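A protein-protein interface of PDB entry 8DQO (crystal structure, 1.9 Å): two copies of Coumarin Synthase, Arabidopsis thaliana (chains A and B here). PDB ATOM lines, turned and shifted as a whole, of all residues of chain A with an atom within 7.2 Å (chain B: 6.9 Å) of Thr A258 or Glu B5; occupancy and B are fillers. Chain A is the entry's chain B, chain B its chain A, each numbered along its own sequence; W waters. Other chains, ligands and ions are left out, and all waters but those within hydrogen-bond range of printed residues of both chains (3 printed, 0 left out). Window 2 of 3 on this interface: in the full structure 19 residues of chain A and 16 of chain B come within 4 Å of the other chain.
The side-chain hydroxyl of Tyr A373 sits at hydrogen-bond distance from the backbone carbonyl oxygen of Thr B7 (3.0 Å).
The backbone NH of Thr A259 lies within hydrogen-bond range of the side-chain carboxylate of Glu B5, 2.7 Å away.
The side-chain carboxylate of Glu B5 is in salt-bridge range of the side-chain amino group of Lys A246 (3.2 Å).
OD1 of Asn B107 is in hydrogen-bond range of OG1 of Thr B3, at 3.2 Å.
The side-chain carboxylate (OD2) of Asp B8 is in hydrogen-bond range of the side-chain amide nitrogen (ND2) of Asn B103.
N of Thr B105 sits at hydrogen-bond distance from O of Glu B5 (2.9 Å).
N of Thr B7 sits at hydrogen-bond distance from O of Asn B103, 2.9 Å away.
OG1 of Thr B7 is in hydrogen-bond range of OD1 of Asp B8 (2.8 Å).
The side-chain amino group (NZ) of Lys A246 lies within hydrogen-bond range of the side-chain hydroxyl (OG1) of Thr A259 (3.0 Å).
Among the printed residues, merely in contact across the chains: Thr A258 with Glu B5 (3.1 Å), Lys A336 with Thr B3 (3.2 Å), Tyr A373 with Ile B6 (3.2 Å) and Tyr A373 with Asp B8 (3.4 Å).
Of the printed residues of chain B, Lys A246 touches Glu B5 (3.2 Å).
Printed residues of chain B within 4 Å of Thr A258: Glu B5.
Of the printed residues of chain B, Thr A259 touches Glu B5 (2.7 Å).
Of the printed residues of chain A, Glu B5 touches Lys A246, Thr A258 and Thr A259.
Thr B105 touches none of the printed residues of chain A.
Val B106 touches none of the printed residues of chain A.
The nearest residue of chain B that does not touch Thr A258 is Thr B3 (5.3 Å).
The nearest residue of chain A that does not touch Glu B5 is Phe A257 (4.2 Å).
Along chain B the printed residues that touch a printed residue of chain A span positions 3 to 8.
Of the 19 printed residues of chain A, 5 touch a printed residue of chain B.
Printed residues of chain A that touch a printed residue of chain B: Lys A246, Thr A258, Thr A259, Lys A336 and Tyr A373.
Among the printed residues, Asp or Glu carboxylates within 4 Å of a Lys or Arg side-chain nitrogen of the other chain: Lys A246 with Glu B5.
No position is printed for both chains.
Of the 7 pairs that touch across the chains among the printed residues, none has its exchanged pair printed and touching as well.
Water W1 bridges NZ of Lys A246 (2.5 Å) and OE1 of Glu B5 (3.1 Å).
Water W2 lies within hydrogen-bond range of the backbone carbonyl oxygen (O) of Ile B6 (2.6 Å), the side-chain carboxylate (OE2) of Glu B5 (2.9 Å), the guanidinium group (NH1) of Arg A372 (3.0 Å) and the side-chain hydroxyl (OG1) of Thr A259 (3.5 Å).
Water W3 lies within hydrogen-bond range of N of Phe A260 (3.0 Å), NH2 of Arg A372 (3.1 Å) and OE2 of Glu B5 (3.3 Å).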
ATOM      1  N   LEU A 242     -12.732 -28.848  18.381  1.00  0.00           N
ATOM      2  CA  LEU A 242     -13.384 -27.587  17.973  1.00  0.00           C
ATOM      3  C   LEU A 242     -13.268 -27.393  16.460  1.00  0.00           C
ATOM      4  O   LEU A 242     -14.205 -26.928  15.823  1.00  0.00           O
ATOM      5  CB  LEU A 242     -12.777 -26.375  18.677  1.00  0.00           C
ATOM      6  CG  LEU A 242     -13.379 -25.989  20.019  1.00  0.00           C
ATOM      7  CD1 LEU A 242     -14.894 -25.967  19.986  1.00  0.00           C
ATOM      8  CD2 LEU A 242     -12.896 -26.915  21.104  1.00  0.00           C
ATOM      9  N   LEU A 245     -15.863 -29.692  14.952  1.00  0.00           N
ATOM     10  CA  LEU A 245     -17.212 -29.123  15.161  1.00  0.00           C
ATOM     11  C   LEU A 245     -17.452 -27.965  14.178  1.00  0.00           C
ATOM     12  O   LEU A 245     -18.476 -27.908  13.537  1.00  0.00           O
ATOM     13  CB  LEU A 245     -17.331 -28.651  16.612  1.00  0.00           C
ATOM     14  CG  LEU A 245     -18.563 -27.805  16.919  1.00  0.00           C
ATOM     15  CD1 LEU A 245     -19.836 -28.643  16.834  1.00  0.00           C
ATOM     16  CD2 LEU A 245     -18.424 -27.163  18.286  1.00  0.00           C
ATOM     17  N   LYS A 246     -16.486 -27.035  14.077  1.00  0.00           N
ATOM     18  CA  LYS A 246     -16.625 -25.858  13.197  1.00  0.00           C
ATOM     19  C   LYS A 246     -16.758 -26.281  11.727  1.00  0.00           C
ATOM     20  O   LYS A 246     -17.561 -25.713  10.973  1.00  0.00           O
ATOM     21  CB  LYS A 246     -15.420 -24.924  13.346  1.00  0.00           C
ATOM     22  CG  LYS A 246     -15.422 -24.060  14.589  1.00  0.00           C
ATOM     23  CD  LYS A 246     -14.183 -23.178  14.597  1.00  0.00           C
ATOM     24  CE  LYS A 246     -13.956 -22.455  15.896  1.00  0.00           C
ATOM     25  NZ  LYS A 246     -12.631 -21.786  15.886  1.00  0.00           N
ATOM     26  N   LEU A 249     -20.256 -27.749  11.222  1.00  0.00           N
ATOM     27  CA  LEU A 249     -21.240 -26.685  11.206  1.00  0.00           C
ATOM     28  C   LEU A 249     -21.210 -25.948   9.860  1.00  0.00           C
ATOM     29  O   LEU A 249     -22.266 -25.697   9.258  1.00  0.00           O
ATOM     30  CB  LEU A 249     -21.000 -25.745  12.390  1.00  0.00           C
ATOM     31  CG  LEU A 249     -21.365 -26.338  13.752  1.00  0.00           C
ATOM     32  CD1 LEU A 249     -20.893 -25.453  14.888  1.00  0.00           C
ATOM     33  CD2 LEU A 249     -22.864 -26.574  13.865  1.00  0.00           C
ATOM     34  N   ASN A 256     -19.386 -19.913   9.162  1.00  0.00           N
ATOM     35  CA  ASN A 256     -18.215 -20.098  10.021  1.00  0.00           C
ATOM     36  C   ASN A 256     -18.545 -19.592  11.420  1.00  0.00           C
ATOM     37  O   ASN A 256     -19.010 -18.478  11.574  1.00  0.00           O
ATOM     38  CB  ASN A 256     -16.986 -19.333   9.532  1.00  0.00           C
ATOM     39  CG  ASN A 256     -16.436 -19.905   8.251  1.00  0.00           C
ATOM     40  OD1 ASN A 256     -16.001 -21.051   8.231  1.00  0.00           O
ATOM     41  ND2 ASN A 256     -16.463 -19.120   7.188  1.00  0.00           N
ATOM     42  N   PHE A 257     -18.317 -20.415  12.436  1.00  0.00           N
ATOM     43  CA  PHE A 257     -18.589 -19.986  13.787  1.00  0.00           C
ATOM     44  C   PHE A 257     -17.258 -19.908  14.541  1.00  0.00           C
ATOM     45  O   PHE A 257     -16.354 -20.702  14.283  1.00  0.00           O
ATOM     46  CB  PHE A 257     -19.563 -20.936  14.473  1.00  0.00           C
ATOM     47  CG  PHE A 257     -20.940 -20.971  13.844  1.00  0.00           C
ATOM     48  CD1 PHE A 257     -21.831 -19.926  14.020  1.00  0.00           C
ATOM     49  CD2 PHE A 257     -21.331 -22.034  13.052  1.00  0.00           C
ATOM     50  CE1 PHE A 257     -23.083 -19.953  13.431  1.00  0.00           C
ATOM     51  CE2 PHE A 257     -22.592 -22.067  12.463  1.00  0.00           C
ATOM     52  CZ  PHE A 257     -23.463 -21.022  12.647  1.00  0.00           C
ATOM     53  N   THR A 258     -17.177 -18.954  15.470  1.00  0.00           N
ATOM     54  CA  THR A 258     -16.083 -18.867  16.418  1.00  0.00           C
ATOM     55  C   THR A 258     -16.263 -20.015  17.413  1.00  0.00           C
ATOM     56  O   THR A 258     -17.421 -20.554  17.575  1.00  0.00           O
ATOM     57  CB  THR A 258     -16.084 -17.526  17.165  1.00  0.00           C
ATOM     58  OG1 THR A 258     -17.240 -17.474  18.003  1.00  0.00           O
ATOM     59  CG2 THR A 258     -16.081 -16.328  16.244  1.00  0.00           C
ATOM     60  N   THR A 259     -15.168 -20.352  18.096  1.00  0.00           N
ATOM     61  CA  THR A 259     -15.187 -21.296  19.198  1.00  0.00           C
ATOM     62  C   THR A 259     -16.288 -20.917  20.198  1.00  0.00           C
ATOM     63  O   THR A 259     -17.072 -21.772  20.610  1.00  0.00           O
ATOM     64  CB  THR A 259     -13.803 -21.414  19.843  1.00  0.00           C
ATOM     65  OG1 THR A 259     -12.981 -22.002  18.835  1.00  0.00           O
ATOM     66  CG2 THR A 259     -13.793 -22.243  21.110  1.00  0.00           C
ATOM     67  N   PHE A 260     -16.360 -19.638  20.564  1.00  0.00           N
ATOM     68  CA  PHE A 260     -17.316 -19.188  21.586  1.00  0.00           C
ATOM     69  C   PHE A 260     -18.763 -19.467  21.153  1.00  0.00           C
ATOM     70  O   PHE A 260     -19.578 -19.915  21.942  1.00  0.00           O
ATOM     71  CB  PHE A 260     -17.091 -17.707  21.867  1.00  0.00           C
ATOM     72  CG  PHE A 260     -17.925 -17.151  22.979  1.00  0.00           C
ATOM     73  CD1 PHE A 260     -17.615 -17.424  24.299  1.00  0.00           C
ATOM     74  CD2 PHE A 260     -19.031 -16.365  22.692  1.00  0.00           C
ATOM     75  CE1 PHE A 260     -18.384 -16.889  25.318  1.00  0.00           C
ATOM     76  CE2 PHE A 260     -19.793 -15.835  23.710  1.00  0.00           C
ATOM     77  CZ  PHE A 260     -19.470 -16.097  25.018  1.00  0.00           C
ATOM     78  N   GLU A 261     -19.058 -19.227  19.878  1.00  0.00           N
ATOM     79  CA  GLU A 261     -20.366 -19.490  19.306  1.00  0.00           C
ATOM     80  C   GLU A 261     -20.700 -20.992  19.316  1.00  0.00           C
ATOM     81  O   GLU A 261     -21.763 -21.382  19.802  1.00  0.00           O
ATOM     82  CB  GLU A 261     -20.431 -18.902  17.902  1.00  0.00           C
ATOM     83  CG  GLU A 261     -20.505 -17.387  17.914  1.00  0.00           C
ATOM     84  CD  GLU A 261     -20.002 -16.689  16.671  1.00  0.00           C
ATOM     85  OE1 GLU A 261     -19.743 -17.387  15.657  1.00  0.00           O
ATOM     86  OE2 GLU A 261     -19.923 -15.441  16.723  1.00  0.00           O
ATOM     87  N   ALA A 262     -19.786 -21.805  18.788  1.00  0.00           N
ATOM     88  CA  ALA A 262     -20.021 -23.222  18.524  1.00  0.00           C
ATOM     89  C   ALA A 262     -20.094 -24.002  19.840  1.00  0.00           C
ATOM     90  O   ALA A 262     -21.063 -24.736  20.077  1.00  0.00           O
ATOM     91  CB  ALA A 262     -18.943 -23.775  17.641  1.00  0.00           C
ATOM     92  N   LEU A 263     -19.039 -23.885  20.650  1.00  0.00           N
ATOM     93  CA  LEU A 263     -18.965 -24.556  21.946  1.00  0.00           C
ATOM     94  C   LEU A 263     -20.012 -23.977  22.909  1.00  0.00           C
ATOM     95  O   LEU A 263     -20.632 -24.739  23.687  1.00  0.00           O
ATOM     96  CB  LEU A 263     -17.545 -24.408  22.503  1.00  0.00           C
ATOM     97  CG  LEU A 263     -17.261 -25.072  23.847  1.00  0.00           C
ATOM     98  CD1 LEU A 263     -17.708 -26.526  23.846  1.00  0.00           C
ATOM     99  CD2 LEU A 263     -15.779 -24.952  24.180  1.00  0.00           C
ATOM    100  N   GLY A 264     -20.194 -22.647  22.869  1.00  0.00           N
ATOM    101  CA  GLY A 264     -21.255 -21.960  23.605  1.00  0.00           C
ATOM    102  C   GLY A 264     -22.624 -22.593  23.350  1.00  0.00           C
ATOM    103  O   GLY A 264     -23.344 -22.904  24.287  1.00  0.00           O
ATOM    104  N   ALA A 329     -25.860 -21.490  17.319  1.00  0.00           N
ATOM    105  CA  ALA A 329     -24.603 -20.759  17.103  1.00  0.00           C
ATOM    106  C   ALA A 329     -24.862 -19.426  16.378  1.00  0.00           C
ATOM    107  O   ALA A 329     -24.251 -18.418  16.735  1.00  0.00           O
ATOM    108  CB  ALA A 329     -23.608 -21.609  16.350  1.00  0.00           C
ATOM    109  N   ILE A 332     -26.302 -16.856  18.839  1.00  0.00           N
ATOM    110  CA  ILE A 332     -25.236 -16.303  19.675  1.00  0.00           C
ATOM    111  C   ILE A 332     -24.425 -15.293  18.841  1.00  0.00           C
ATOM    112  O   ILE A 332     -24.118 -14.199  19.328  1.00  0.00           O
ATOM    113  CB  ILE A 332     -24.380 -17.435  20.291  1.00  0.00           C
ATOM    114  CG1 ILE A 332     -25.202 -18.280  21.273  1.00  0.00           C
ATOM    115  CG2 ILE A 332     -23.121 -16.898  20.963  1.00  0.00           C
ATOM    116  CD1 ILE A 332     -24.561 -19.588  21.672  1.00  0.00           C
ATOM    117  N   LYS A 333     -24.081 -15.651  17.596  1.00  0.00           N
ATOM    118  CA  LYS A 333     -23.340 -14.754  16.714  1.00  0.00           C
ATOM    119  C   LYS A 333     -24.096 -13.427  16.521  1.00  0.00           C
ATOM    120  O   LYS A 333     -23.514 -12.349  16.619  1.00  0.00           O
ATOM    121  CB  LYS A 333     -23.108 -15.406  15.353  1.00  0.00           C
ATOM    122  CG  LYS A 333     -22.322 -14.564  14.363  1.00  0.00           C
ATOM    123  CD  LYS A 333     -22.420 -15.070  12.955  1.00  0.00           C
ATOM    124  CE  LYS A 333     -21.566 -16.286  12.702  1.00  0.00           C
ATOM    125  NZ  LYS A 333     -21.999 -16.981  11.466  1.00  0.00           N
ATOM    126  N   LYS A 336     -24.174 -10.193  19.049  1.00  0.00           N
ATOM    127  CA  LYS A 336     -23.140  -9.150  19.030  1.00  0.00           C
ATOM    128  C   LYS A 336     -23.597  -7.920  18.231  1.00  0.00           C
ATOM    129  O   LYS A 336     -23.037  -6.826  18.410  1.00  0.00           O
ATOM    130  CB  LYS A 336     -21.831  -9.700  18.455  1.00  0.00           C
ATOM    131  CG  LYS A 336     -20.588  -8.943  18.899  1.00  0.00           C
ATOM    132  CD  LYS A 336     -19.385  -9.830  19.157  1.00  0.00           C
ATOM    133  CE  LYS A 336     -19.016 -10.720  17.984  1.00  0.00           C
ATOM    134  NZ  LYS A 336     -17.652 -11.292  18.158  1.00  0.00           N
ATOM    135  N   ARG A 372      -9.868 -17.154  28.149  1.00  0.00           N
ATOM    136  CA  ARG A 372      -8.743 -17.844  27.545  1.00  0.00           C
ATOM    137  C   ARG A 372      -7.558 -16.893  27.318  1.00  0.00           C
ATOM    138  O   ARG A 372      -6.435 -17.271  27.579  1.00  0.00           O
ATOM    139  CB  ARG A 372      -9.144 -18.506  26.225  1.00  0.00           C
ATOM    140  CG  ARG A 372      -9.897 -19.817  26.402  1.00  0.00           C
ATOM    141  CD  ARG A 372     -10.355 -20.358  25.062  1.00  0.00           C
ATOM    142  NE  ARG A 372     -11.368 -19.492  24.480  1.00  0.00           N
ATOM    143  CZ  ARG A 372     -11.749 -19.496  23.199  1.00  0.00           C
ATOM    144  NH1 ARG A 372     -11.193 -20.328  22.331  1.00  0.00           N
ATOM    145  NH2 ARG A 372     -12.673 -18.640  22.792  1.00  0.00           N
ATOM    146  N   TYR A 373      -7.823 -15.683  26.816  1.00  0.00           N
ATOM    147  CA  TYR A 373      -6.775 -14.850  26.241  1.00  0.00           C
ATOM    148  C   TYR A 373      -6.690 -13.517  26.997  1.00  0.00           C
ATOM    149  O   TYR A 373      -6.374 -12.481  26.422  1.00  0.00           O
ATOM    150  CB  TYR A 373      -7.033 -14.707  24.737  1.00  0.00           C
ATOM    151  CG  TYR A 373      -7.184 -16.025  24.017  1.00  0.00           C
ATOM    152  CD1 TYR A 373      -6.229 -17.021  24.146  1.00  0.00           C
ATOM    153  CD2 TYR A 373      -8.292 -16.288  23.221  1.00  0.00           C
ATOM    154  CE1 TYR A 373      -6.363 -18.240  23.506  1.00  0.00           C
ATOM    155  CE2 TYR A 373      -8.431 -17.495  22.557  1.00  0.00           C
ATOM    156  CZ  TYR A 373      -7.469 -18.476  22.707  1.00  0.00           C
ATOM    157  OH  TYR A 373      -7.611 -19.678  22.084  1.00  0.00           O
ATOM    158  N   THR B   3     -15.234  -9.333  13.049  1.00  0.00           N
ATOM    159  CA  THR B   3     -14.802 -10.040  14.244  1.00  0.00           C
ATOM    160  C   THR B   3     -13.459 -10.731  13.978  1.00  0.00           C
ATOM    161  O   THR B   3     -13.334 -11.505  13.034  1.00  0.00           O
ATOM    162  CB  THR B   3     -15.872 -11.050  14.660  1.00  0.00           C
ATOM    163  OG1 THR B   3     -16.134 -11.840  13.501  1.00  0.00           O
ATOM    164  CG2 THR B   3     -17.154 -10.402  15.138  1.00  0.00           C
ATOM    165  N   LEU B   4     -12.463 -10.438  14.816  1.00  0.00           N
ATOM    166  CA  LEU B   4     -11.213 -11.157  14.814  1.00  0.00           C
ATOM    167  C   LEU B   4     -11.313 -12.224  15.916  1.00  0.00           C
ATOM    168  O   LEU B   4     -11.548 -11.891  17.067  1.00  0.00           O
ATOM    169  CB  LEU B   4     -10.069 -10.150  15.026  1.00  0.00           C
ATOM    170  CG  LEU B   4      -8.658 -10.738  15.042  1.00  0.00           C
ATOM    171  CD1 LEU B   4      -7.647  -9.798  14.412  1.00  0.00           C
ATOM    172  CD2 LEU B   4      -8.242 -11.096  16.456  1.00  0.00           C
ATOM    173  N   GLU B   5     -11.206 -13.507  15.546  1.00  0.00           N
ATOM    174  CA  GLU B   5     -11.262 -14.645  16.507  1.00  0.00           C
ATOM    175  C   GLU B   5      -9.865 -15.254  16.731  1.00  0.00           C
ATOM    176  O   GLU B   5      -9.095 -15.636  15.722  1.00  0.00           O
ATOM    177  CB  GLU B   5     -12.082 -15.826  15.967  1.00  0.00           C
ATOM    178  CG  GLU B   5     -12.157 -17.001  16.950  1.00  0.00           C
ATOM    179  CD  GLU B   5     -12.974 -18.103  16.455  1.00  0.00           C
ATOM    180  OE1 GLU B   5     -13.353 -18.001  15.262  1.00  0.00           O
ATOM    181  OE2 GLU B   5     -13.079 -18.943  17.234  1.00  0.00           O
ATOM    182  N   ILE B   6      -9.390 -15.192  18.010  1.00  0.00           N
ATOM    183  CA  ILE B   6      -8.113 -15.836  18.390  1.00  0.00           C
ATOM    184  C   ILE B   6      -8.447 -17.315  18.552  1.00  0.00           C
ATOM    185  O   ILE B   6      -9.167 -17.676  19.465  1.00  0.00           O
ATOM    186  CB  ILE B   6      -7.472 -15.260  19.668  1.00  0.00           C
ATOM    187  CG1 ILE B   6      -6.942 -13.839  19.454  1.00  0.00           C
ATOM    188  CG2 ILE B   6      -6.371 -16.187  20.166  1.00  0.00           C
ATOM    189  CD1 ILE B   6      -6.352 -13.199  20.694  1.00  0.00           C
ATOM    190  N   THR B   7      -7.937 -18.139  17.641  1.00  0.00           N
ATOM    191  CA  THR B   7      -8.225 -19.554  17.660  1.00  0.00           C
ATOM    192  C   THR B   7      -7.360 -20.238  18.728  1.00  0.00           C
ATOM    193  O   THR B   7      -7.831 -21.086  19.424  1.00  0.00           O
ATOM    194  CB  THR B   7      -8.056 -20.174  16.267  1.00  0.00           C
ATOM    195  OG1 THR B   7      -6.698 -20.105  15.839  1.00  0.00           O
ATOM    196  CG2 THR B   7      -8.901 -19.484  15.222  1.00  0.00           C
ATOM    197  N   ASP B   8      -6.077 -19.831  18.850  1.00  0.00           N
ATOM    198  CA  ASP B   8      -5.165 -20.475  19.810  1.00  0.00           C
ATOM    199  C   ASP B   8      -3.865 -19.659  19.968  1.00  0.00           C
ATOM    200  O   ASP B   8      -3.519 -18.782  19.133  1.00  0.00           O
ATOM    201  CB  ASP B   8      -4.884 -21.920  19.375  1.00  0.00           C
ATOM    202  CG  ASP B   8      -4.218 -21.978  18.011  1.00  0.00           C
ATOM    203  OD1 ASP B   8      -4.968 -22.016  16.952  1.00  0.00           O
ATOM    204  OD2 ASP B   8      -2.973 -21.873  18.017  1.00  0.00           O
ATOM    205  N   ASN B 103      -2.482 -17.180  16.976  1.00  0.00           N
ATOM    206  CA  ASN B 103      -3.155 -17.560  15.732  1.00  0.00           C
ATOM    207  C   ASN B 103      -4.581 -17.014  15.747  1.00  0.00           C
ATOM    208  O   ASN B 103      -5.340 -17.302  16.674  1.00  0.00           O
ATOM    209  CB  ASN B 103      -3.169 -19.064  15.498  1.00  0.00           C
ATOM    210  CG  ASN B 103      -1.786 -19.610  15.239  1.00  0.00           C
ATOM    211  OD1 ASN B 103      -1.113 -19.172  14.309  1.00  0.00           O
ATOM    212  ND2 ASN B 103      -1.360 -20.554  16.065  1.00  0.00           N
ATOM    213  N   ALA B 104      -4.933 -16.289  14.685  1.00  0.00           N
ATOM    214  CA  ALA B 104      -6.221 -15.581  14.580  1.00  0.00           C
ATOM    215  C   ALA B 104      -6.809 -15.692  13.155  1.00  0.00           C
ATOM    216  O   ALA B 104      -6.183 -16.096  12.168  1.00  0.00           O
ATOM    217  CB  ALA B 104      -6.034 -14.140  15.015  1.00  0.00           C
ATOM    218  N   THR B 105      -8.094 -15.321  13.066  1.00  0.00           N
ATOM    219  CA  THR B 105      -8.803 -15.346  11.806  1.00  0.00           C
ATOM    220  C   THR B 105      -9.956 -14.285  11.828  1.00  0.00           C
ATOM    221  O   THR B 105     -10.458 -13.930  12.761  1.00  0.00           O
ATOM    222  CB  THR B 105      -9.380 -16.740  11.550  1.00  0.00           C
ATOM    223  OG1 THR B 105      -9.957 -16.719  10.243  1.00  0.00           O
ATOM    224  CG2 THR B 105     -10.429 -17.105  12.578  1.00  0.00           C
ATOM    225  N   VAL B 106      -9.958 -13.512  10.698  1.00  0.00           N
ATOM    226  CA  VAL B 106     -10.926 -12.449  10.577  1.00  0.00           C
ATOM    227  C   VAL B 106     -11.739 -12.645   9.287  1.00  0.00           C
ATOM    228  O   VAL B 106     -11.287 -13.251   8.324  1.00  0.00           O
ATOM    229  CB  VAL B 106     -10.274 -11.056  10.709  1.00  0.00           C
ATOM    230  CG1 VAL B 106      -9.042 -10.866   9.828  1.00  0.00           C
ATOM    231  CG2 VAL B 106     -11.297  -9.947  10.480  1.00  0.00           C
ATOM    232  N   ASN B 107     -12.982 -12.156   9.328  1.00  0.00           N
ATOM    233  CA  ASN B 107     -13.906 -12.143   8.178  1.00  0.00           C
ATOM    234  C   ASN B 107     -13.823 -10.778   7.473  1.00  0.00           C
ATOM    235  O   ASN B 107     -14.651  -9.890   7.710  1.00  0.00           O
ATOM    236  CB  ASN B 107     -15.332 -12.500   8.615  1.00  0.00           C
ATOM    237  CG  ASN B 107     -15.899 -11.643   9.734  1.00  0.00           C
ATOM    238  OD1 ASN B 107     -16.899 -12.009  10.348  1.00  0.00           O
ATOM    239  ND2 ASN B 107     -15.299 -10.497  10.008  1.00  0.00           N
ATOM    240  N   THR B 146      -2.478 -13.741  11.568  1.00  0.00           N
ATOM    241  CA  THR B 146      -3.917 -13.529  11.362  1.00  0.00           C
ATOM    242  C   THR B 146      -4.249 -13.831   9.901  1.00  0.00           C
ATOM    243  O   THR B 146      -3.682 -13.199   9.000  1.00  0.00           O
ATOM    244  CB  THR B 146      -4.374 -12.101  11.683  1.00  0.00           C
ATOM    245  OG1 THR B 146      -3.931 -11.699  12.982  1.00  0.00           O
ATOM    246  CG2 THR B 146      -5.883 -11.969  11.639  1.00  0.00           C
HETATM  247  O   HOH W   1     -12.390 -20.559  13.733  1.00  0.00           O
HETATM  248  O   HOH W   2     -11.415 -18.996  19.608  1.00  0.00           O
HETATM  249  O   HOH W   3     -14.089 -17.744  20.170  1.00  0.00           O
